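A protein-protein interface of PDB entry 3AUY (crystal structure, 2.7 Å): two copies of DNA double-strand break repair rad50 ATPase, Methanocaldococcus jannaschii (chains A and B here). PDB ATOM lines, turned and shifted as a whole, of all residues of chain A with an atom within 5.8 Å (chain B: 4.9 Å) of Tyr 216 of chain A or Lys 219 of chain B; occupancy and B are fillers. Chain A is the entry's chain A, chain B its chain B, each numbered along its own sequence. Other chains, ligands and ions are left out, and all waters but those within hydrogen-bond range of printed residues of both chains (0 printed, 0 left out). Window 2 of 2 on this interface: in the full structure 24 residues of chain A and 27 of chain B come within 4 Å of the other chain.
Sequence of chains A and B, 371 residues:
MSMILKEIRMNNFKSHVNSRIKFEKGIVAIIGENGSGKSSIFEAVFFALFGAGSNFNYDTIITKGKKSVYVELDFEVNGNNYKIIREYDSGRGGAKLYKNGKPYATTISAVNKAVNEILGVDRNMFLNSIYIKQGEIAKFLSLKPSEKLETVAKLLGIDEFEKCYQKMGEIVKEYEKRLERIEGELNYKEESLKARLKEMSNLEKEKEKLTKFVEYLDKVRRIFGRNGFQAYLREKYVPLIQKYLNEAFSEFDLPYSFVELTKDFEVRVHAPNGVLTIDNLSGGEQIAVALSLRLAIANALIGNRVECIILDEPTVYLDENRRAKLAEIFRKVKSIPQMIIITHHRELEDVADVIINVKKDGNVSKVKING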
ATOM      1  N   LYS A 212       7.044 -12.252 -25.385  1.00  0.00           N
ATOM      2  CA  LYS A 212       6.221 -13.062 -24.505  1.00  0.00           C
ATOM      3  C   LYS A 212       7.098 -14.161 -23.915  1.00  0.00           C
ATOM      4  O   LYS A 212       7.166 -14.307 -22.699  1.00  0.00           O
ATOM      5  CB  LYS A 212       5.064 -13.676 -25.295  1.00  0.00           C
ATOM      6  CG  LYS A 212       4.125 -14.547 -24.484  1.00  0.00           C
ATOM      7  CD  LYS A 212       3.249 -15.382 -25.405  1.00  0.00           C
ATOM      8  CE  LYS A 212       2.546 -16.501 -24.647  1.00  0.00           C
ATOM      9  NZ  LYS A 212       1.845 -17.442 -25.563  1.00  0.00           N
ATOM     10  N   PHE A 213       7.765 -14.935 -24.772  1.00  0.00           N
ATOM     11  CA  PHE A 213       8.643 -16.002 -24.293  1.00  0.00           C
ATOM     12  C   PHE A 213       9.727 -15.427 -23.388  1.00  0.00           C
ATOM     13  O   PHE A 213      10.108 -16.057 -22.408  1.00  0.00           O
ATOM     14  CB  PHE A 213       9.345 -16.737 -25.442  1.00  0.00           C
ATOM     15  CG  PHE A 213       8.426 -17.485 -26.363  1.00  0.00           C
ATOM     16  CD1 PHE A 213       7.069 -17.606 -26.089  1.00  0.00           C
ATOM     17  CD2 PHE A 213       8.925 -18.061 -27.523  1.00  0.00           C
ATOM     18  CE1 PHE A 213       6.226 -18.290 -26.964  1.00  0.00           C
ATOM     19  CE2 PHE A 213       8.090 -18.742 -28.396  1.00  0.00           C
ATOM     20  CZ  PHE A 213       6.739 -18.854 -28.116  1.00  0.00           C
ATOM     21  N   VAL A 214      10.233 -14.240 -23.721  1.00  0.00           N
ATOM     22  CA  VAL A 214      11.282 -13.626 -22.912  1.00  0.00           C
ATOM     23  C   VAL A 214      10.815 -13.510 -21.466  1.00  0.00           C
ATOM     24  O   VAL A 214      11.530 -13.905 -20.550  1.00  0.00           O
ATOM     25  CB  VAL A 214      11.690 -12.219 -23.442  1.00  0.00           C
ATOM     26  CG1 VAL A 214      10.566 -11.218 -23.215  1.00  0.00           C
ATOM     27  CG2 VAL A 214      12.954 -11.749 -22.757  1.00  0.00           C
ATOM     28  N   GLU A 215       9.609 -12.991 -21.262  1.00  0.00           N
ATOM     29  CA  GLU A 215       9.077 -12.847 -19.915  1.00  0.00           C
ATOM     30  C   GLU A 215       9.045 -14.201 -19.221  1.00  0.00           C
ATOM     31  O   GLU A 215       9.457 -14.326 -18.071  1.00  0.00           O
ATOM     32  CB  GLU A 215       7.664 -12.265 -19.942  1.00  0.00           C
ATOM     33  CG  GLU A 215       7.079 -12.087 -18.546  1.00  0.00           C
ATOM     34  CD  GLU A 215       5.582 -11.820 -18.559  1.00  0.00           C
ATOM     35  OE1 GLU A 215       5.155 -10.776 -19.107  1.00  0.00           O
ATOM     36  OE2 GLU A 215       4.829 -12.664 -18.023  1.00  0.00           O
ATOM     37  N   TYR A 216       8.540 -15.207 -19.923  1.00  0.00           N
ATOM     38  CA  TYR A 216       8.464 -16.548 -19.374  1.00  0.00           C
ATOM     39  C   TYR A 216       9.836 -16.990 -18.937  1.00  0.00           C
ATOM     40  O   TYR A 216      10.084 -17.188 -17.750  1.00  0.00           O
ATOM     41  CB  TYR A 216       7.941 -17.519 -20.418  1.00  0.00           C
ATOM     42  CG  TYR A 216       6.504 -17.289 -20.777  1.00  0.00           C
ATOM     43  CD1 TYR A 216       5.932 -17.935 -21.877  1.00  0.00           C
ATOM     44  CD2 TYR A 216       5.704 -16.436 -20.015  1.00  0.00           C
ATOM     45  CE1 TYR A 216       4.599 -17.736 -22.211  1.00  0.00           C
ATOM     46  CE2 TYR A 216       4.370 -16.229 -20.334  1.00  0.00           C
ATOM     47  CZ  TYR A 216       3.820 -16.882 -21.435  1.00  0.00           C
ATOM     48  OH  TYR A 216       2.491 -16.688 -21.752  1.00  0.00           O
ATOM     49  N   LEU A 217      10.725 -17.149 -19.906  1.00  0.00           N
ATOM     50  CA  LEU A 217      12.075 -17.564 -19.611  1.00  0.00           C
ATOM     51  C   LEU A 217      12.608 -16.842 -18.387  1.00  0.00           C
ATOM     52  O   LEU A 217      13.119 -17.474 -17.468  1.00  0.00           O
ATOM     53  CB  LEU A 217      12.997 -17.291 -20.795  1.00  0.00           C
ATOM     54  CG  LEU A 217      12.813 -18.176 -22.026  1.00  0.00           C
ATOM     55  CD1 LEU A 217      13.804 -17.744 -23.079  1.00  0.00           C
ATOM     56  CD2 LEU A 217      13.013 -19.634 -21.675  1.00  0.00           C
ATOM     57  N   ASP A 218      12.474 -15.523 -18.346  1.00  0.00           N
ATOM     58  CA  ASP A 218      13.011 -14.807 -17.206  1.00  0.00           C
ATOM     59  C   ASP A 218      12.485 -15.310 -15.883  1.00  0.00           C
ATOM     60  O   ASP A 218      13.207 -15.359 -14.889  1.00  0.00           O
ATOM     61  CB  ASP A 218      12.751 -13.315 -17.300  1.00  0.00           C
ATOM     62  CG  ASP A 218      13.658 -12.536 -16.373  1.00  0.00           C
ATOM     63  OD1 ASP A 218      14.898 -12.726 -16.463  1.00  0.00           O
ATOM     64  OD2 ASP A 218      13.140 -11.752 -15.545  1.00  0.00           O
ATOM     65  N   LYS A 219      11.222 -15.693 -15.856  1.00  0.00           N
ATOM     66  CA  LYS A 219      10.672 -16.185 -14.620  1.00  0.00           C
ATOM     67  C   LYS A 219      11.222 -17.561 -14.290  1.00  0.00           C
ATOM     68  O   LYS A 219      11.606 -17.831 -13.146  1.00  0.00           O
ATOM     69  CB  LYS A 219       9.157 -16.210 -14.697  1.00  0.00           C
ATOM     70  CG  LYS A 219       8.546 -14.916 -14.242  1.00  0.00           C
ATOM     71  CD  LYS A 219       7.127 -14.790 -14.745  1.00  0.00           C
ATOM     72  CE  LYS A 219       6.729 -13.329 -14.882  1.00  0.00           C
ATOM     73  NZ  LYS A 219       5.645 -13.160 -15.883  1.00  0.00           N
ATOM     74  N   VAL A 220      11.278 -18.431 -15.288  1.00  0.00           N
ATOM     75  CA  VAL A 220      11.771 -19.770 -15.046  1.00  0.00           C
ATOM     76  C   VAL A 220      13.278 -19.705 -14.865  1.00  0.00           C
ATOM     77  O   VAL A 220      13.884 -20.632 -14.346  1.00  0.00           O
ATOM     78  CB  VAL A 220      11.369 -20.725 -16.189  1.00  0.00           C
ATOM     79  CG1 VAL A 220      11.801 -20.156 -17.496  1.00  0.00           C
ATOM     80  CG2 VAL A 220      11.991 -22.078 -15.994  1.00  0.00           C
ATOM     81  N   ARG A 221      13.881 -18.592 -15.270  1.00  0.00           N
ATOM     82  CA  ARG A 221      15.328 -18.423 -15.116  1.00  0.00           C
ATOM     83  C   ARG A 221      15.615 -18.105 -13.646  1.00  0.00           C
ATOM     84  O   ARG A 221      16.623 -18.528 -13.086  1.00  0.00           O
ATOM     85  CB  ARG A 221      15.839 -17.289 -16.025  1.00  0.00           C
ATOM     86  CG  ARG A 221      17.305 -16.919 -15.834  1.00  0.00           C
ATOM     87  CD  ARG A 221      17.727 -15.841 -16.823  1.00  0.00           C
ATOM     88  NE  ARG A 221      18.812 -14.978 -16.335  1.00  0.00           N
ATOM     89  CZ  ARG A 221      20.100 -15.317 -16.279  1.00  0.00           C
ATOM     90  NH1 ARG A 221      20.502 -16.514 -16.680  1.00  0.00           N
ATOM     91  NH2 ARG A 221      20.998 -14.448 -15.826  1.00  0.00           N
ATOM     92  N   GLU B 215       3.688 -22.942 -12.551  1.00  0.00           N
ATOM     93  CA  GLU B 215       3.013 -22.349 -13.691  1.00  0.00           C
ATOM     94  C   GLU B 215       4.029 -21.889 -14.729  1.00  0.00           C
ATOM     95  O   GLU B 215       3.980 -22.310 -15.882  1.00  0.00           O
ATOM     96  CB  GLU B 215       2.182 -21.164 -13.206  1.00  0.00           C
ATOM     97  CG  GLU B 215       1.302 -20.503 -14.237  1.00  0.00           C
ATOM     98  CD  GLU B 215       0.565 -19.331 -13.635  1.00  0.00           C
ATOM     99  OE1 GLU B 215      -0.008 -19.503 -12.535  1.00  0.00           O
ATOM    100  OE2 GLU B 215       0.562 -18.243 -14.253  1.00  0.00           O
ATOM    101  N   TYR B 216       4.943 -21.011 -14.322  1.00  0.00           N
ATOM    102  CA  TYR B 216       5.945 -20.524 -15.245  1.00  0.00           C
ATOM    103  C   TYR B 216       6.671 -21.729 -15.818  1.00  0.00           C
ATOM    104  O   TYR B 216       6.878 -21.830 -17.028  1.00  0.00           O
ATOM    105  CB  TYR B 216       6.953 -19.624 -14.543  1.00  0.00           C
ATOM    106  CG  TYR B 216       6.362 -18.520 -13.705  1.00  0.00           C
ATOM    107  CD1 TYR B 216       5.301 -17.739 -14.177  1.00  0.00           C
ATOM    108  CD2 TYR B 216       6.898 -18.222 -12.447  1.00  0.00           C
ATOM    109  CE1 TYR B 216       4.791 -16.685 -13.411  1.00  0.00           C
ATOM    110  CE2 TYR B 216       6.400 -17.172 -11.674  1.00  0.00           C
ATOM    111  CZ  TYR B 216       5.350 -16.409 -12.160  1.00  0.00           C
ATOM    112  OH  TYR B 216       4.868 -15.369 -11.399  1.00  0.00           O
ATOM    113  N   LEU B 217       7.052 -22.652 -14.944  1.00  0.00           N
ATOM    114  CA  LEU B 217       7.759 -23.849 -15.378  1.00  0.00           C
ATOM    115  C   LEU B 217       7.018 -24.640 -16.461  1.00  0.00           C
ATOM    116  O   LEU B 217       7.633 -25.110 -17.409  1.00  0.00           O
ATOM    117  CB  LEU B 217       8.081 -24.742 -14.175  1.00  0.00           C
ATOM    118  CG  LEU B 217       9.345 -24.310 -13.438  1.00  0.00           C
ATOM    119  CD1 LEU B 217       9.453 -25.004 -12.107  1.00  0.00           C
ATOM    120  CD2 LEU B 217      10.535 -24.620 -14.312  1.00  0.00           C
ATOM    121  N   ASP B 218       5.706 -24.796 -16.345  1.00  0.00           N
ATOM    122  CA  ASP B 218       5.006 -25.521 -17.395  1.00  0.00           C
ATOM    123  C   ASP B 218       4.884 -24.687 -18.673  1.00  0.00           C
ATOM    124  O   ASP B 218       4.909 -25.241 -19.781  1.00  0.00           O
ATOM    125  CB  ASP B 218       3.642 -26.022 -16.912  1.00  0.00           C
ATOM    126  CG  ASP B 218       3.755 -27.349 -16.166  1.00  0.00           C
ATOM    127  OD1 ASP B 218       4.804 -28.015 -16.314  1.00  0.00           O
ATOM    128  OD2 ASP B 218       2.806 -27.731 -15.446  1.00  0.00           O
ATOM    129  N   LYS B 219       4.775 -23.363 -18.534  1.00  0.00           N
ATOM    130  CA  LYS B 219       4.708 -22.509 -19.717  1.00  0.00           C
ATOM    131  C   LYS B 219       5.970 -22.729 -20.559  1.00  0.00           C
ATOM    132  O   LYS B 219       5.885 -23.017 -21.753  1.00  0.00           O
ATOM    133  CB  LYS B 219       4.606 -21.030 -19.346  1.00  0.00           C
ATOM    134  CG  LYS B 219       3.193 -20.529 -19.136  1.00  0.00           C
ATOM    135  CD  LYS B 219       3.155 -19.008 -19.161  1.00  0.00           C
ATOM    136  CE  LYS B 219       1.811 -18.471 -18.698  1.00  0.00           C
ATOM    137  NZ  LYS B 219       1.575 -18.752 -17.249  1.00  0.00           N
ATOM    138  N   VAL B 220       7.145 -22.602 -19.950  1.00  0.00           N
ATOM    139  CA  VAL B 220       8.364 -22.814 -20.714  1.00  0.00           C
ATOM    140  C   VAL B 220       8.524 -24.294 -21.051  1.00  0.00           C
ATOM    141  O   VAL B 220       8.995 -24.636 -22.130  1.00  0.00           O
ATOM    142  CB  VAL B 220       9.621 -22.303 -19.952  1.00  0.00           C
ATOM    143  CG1 VAL B 220      10.887 -22.695 -20.694  1.00  0.00           C
ATOM    144  CG2 VAL B 220       9.557 -20.784 -19.818  1.00  0.00           C
ATOM    145  N   ARG B 221       8.103 -25.174 -20.145  1.00  0.00           N
ATOM    146  CA  ARG B 221       8.236 -26.615 -20.376  1.00  0.00           C
ATOM    147  C   ARG B 221       7.543 -27.085 -21.647  1.00  0.00           C
ATOM    148  O   ARG B 221       8.015 -28.016 -22.298  1.00  0.00           O
ATOM    149  CB  ARG B 221       7.702 -27.414 -19.187  1.00  0.00           C
ATOM    150  CG  ARG B 221       8.739 -28.336 -18.564  1.00  0.00           C
ATOM    151  CD  ARG B 221       8.142 -29.169 -17.425  1.00  0.00           C
ATOM    152  NE  ARG B 221       7.872 -30.552 -17.816  1.00  0.00           N
ATOM    153  CZ  ARG B 221       8.811 -31.426 -18.169  1.00  0.00           C
ATOM    154  NH1 ARG B 221      10.091 -31.062 -18.181  1.00  0.00           N
ATOM    155  NH2 ARG B 221       8.472 -32.666 -18.504  1.00  0.00           N
ATOM    156  N   ARG B 222       6.423 -26.452 -21.997  1.00  0.00           N
ATOM    157  CA  ARG B 222       5.693 -26.825 -23.206  1.00  0.00           C
ATOM    158  C   ARG B 222       6.193 -26.014 -24.399  1.00  0.00           C
ATOM    159  O   ARG B 222       6.475 -26.574 -25.449  1.00  0.00           O
ATOM    160  CB  ARG B 222       4.178 -26.630 -23.017  1.00  0.00           C
ATOM    161  CG  ARG B 222       3.697 -25.175 -22.895  1.00  0.00           C
ATOM    162  CD  ARG B 222       2.164 -25.104 -22.756  1.00  0.00           C
ATOM    163  NE  ARG B 222       1.710 -25.618 -21.465  1.00  0.00           N
ATOM    164  CZ  ARG B 222       1.433 -24.849 -20.414  1.00  0.00           C
ATOM    165  NH1 ARG B 222       1.553 -23.528 -20.510  1.00  0.00           N
ATOM    166  NH2 ARG B 222       1.062 -25.397 -19.258  1.00  0.00           N
ATOM    167  N   ILE B 223       6.317 -24.702 -24.229  1.00  0.00           N
ATOM    168  CA  ILE B 223       6.800 -23.826 -25.290  1.00  0.00           C
ATOM    169  C   ILE B 223       8.225 -24.197 -25.737  1.00  0.00           C
ATOM    170  O   ILE B 223       8.777 -23.568 -26.631  1.00  0.00           O
ATOM    171  CB  ILE B 223       6.741 -22.330 -24.825  1.00  0.00           C
ATOM    172  CG1 ILE B 223       5.283 -21.857 -24.824  1.00  0.00           C
ATOM    173  CG2 ILE B 223       7.605 -21.427 -25.720  1.00  0.00           C
ATOM    174  CD1 ILE B 223       5.096 -20.377 -24.506  1.00  0.00           C
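Of the 9 printed residues of chain B, 5 touch a printed residue of chain A. Hydrophobic or aromatic side chains of chain B that line the printed part of chain A: Tyr 216, Leu 217, Val 220 and Ile 223. Of the 10 printed residues of chain A, 5 touch a printed residue of chain B. Printed residues of chain A that touch a printed residue of chain B: Phe 213, Tyr 216, Leu 217, Lys 219 and Val 220. Hydrophobic or aromatic side chains of chain A within 4 Å of the printed part of chain B: Phe 213, Tyr 216, Leu 217 and Val 220. Among the printed residues, no Asp or Glu carboxylate lies within 4 Å of a Lys or Arg side-chain nitrogen of the other chain.
Printed residues of chain B within 4 Å of Tyr 216 of chain A: Lys 219, Val 220 and Ile 223. Printed residues of chain A within 4 Å of Lys 219 of chain B: Tyr 216. Of the printed residues of chain A, Val 220 of chain B touches Tyr 216, Leu 217 and Val 220. Of the printed residues of chain B, Lys 219 of chain A touches Tyr 216. Of the printed residues of chain A, Ile 223 of chain B touches Phe 213 and Tyr 216. Of the printed residues of chain A, Tyr 216 of chain B touches Lys 219. Arg 221 of chain A touches none of the printed residues of chain B. The nearest printed residue of chain B that does not touch Tyr 216 of chain A is Tyr 216 of chain B (5.1 Å). The nearest printed residue of chain A that does not touch Leu 217 of chain B is Lys 219 of chain A (6.6 Å).
Tyr 216 of chain A touches Lys 219 of chain B, and with the chains exchanged Lys 219 of chain A touches Tyr 216 of chain B. Tyr 216 of chain A touches Val 220 of chain B, but with the chains exchanged Val 220 of chain A does not touch Tyr 216 of chain B (4.5 Å). Leu 217 of chain A touches Val 220 of chain B, and with the chains exchanged Val 220 of chain A touches Leu 217 of chain B. Val 220 of chain A touches its own counterpart, Val 220 of chain B. Of the 8 pairs that touch across the chains among the printed residues, 5 have their exchanged pair printed and touching as well.
The side-chain carboxylate of Glu 215 of chain B is in salt-bridge range of the side-chain amino group of Lys 219 of chain B, 3.2 Å away.
Phe 213 of chain A touches Ile 223 of chain B (CE1 to CD1, 3.4 Å). Tyr 216 of chain A touches Lys 219 of chain B. Val 220 of chain B touches Tyr 216 of chain A (CG2 to CB, 3.7 Å). CE1 of Tyr 216 of chain A touches CD1 of Ile 223 of chain B, at 3.5 Å. Leu 217 of chain A touches Val 220 of chain B. Tyr 216 of chain B touches Lys 219 of chain A. Val 220 of chain A touches Leu 217 of chain B. CG1 of Val 220 of chain A touches CG2 of Val 220 of chain B, at 3.3 Å.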
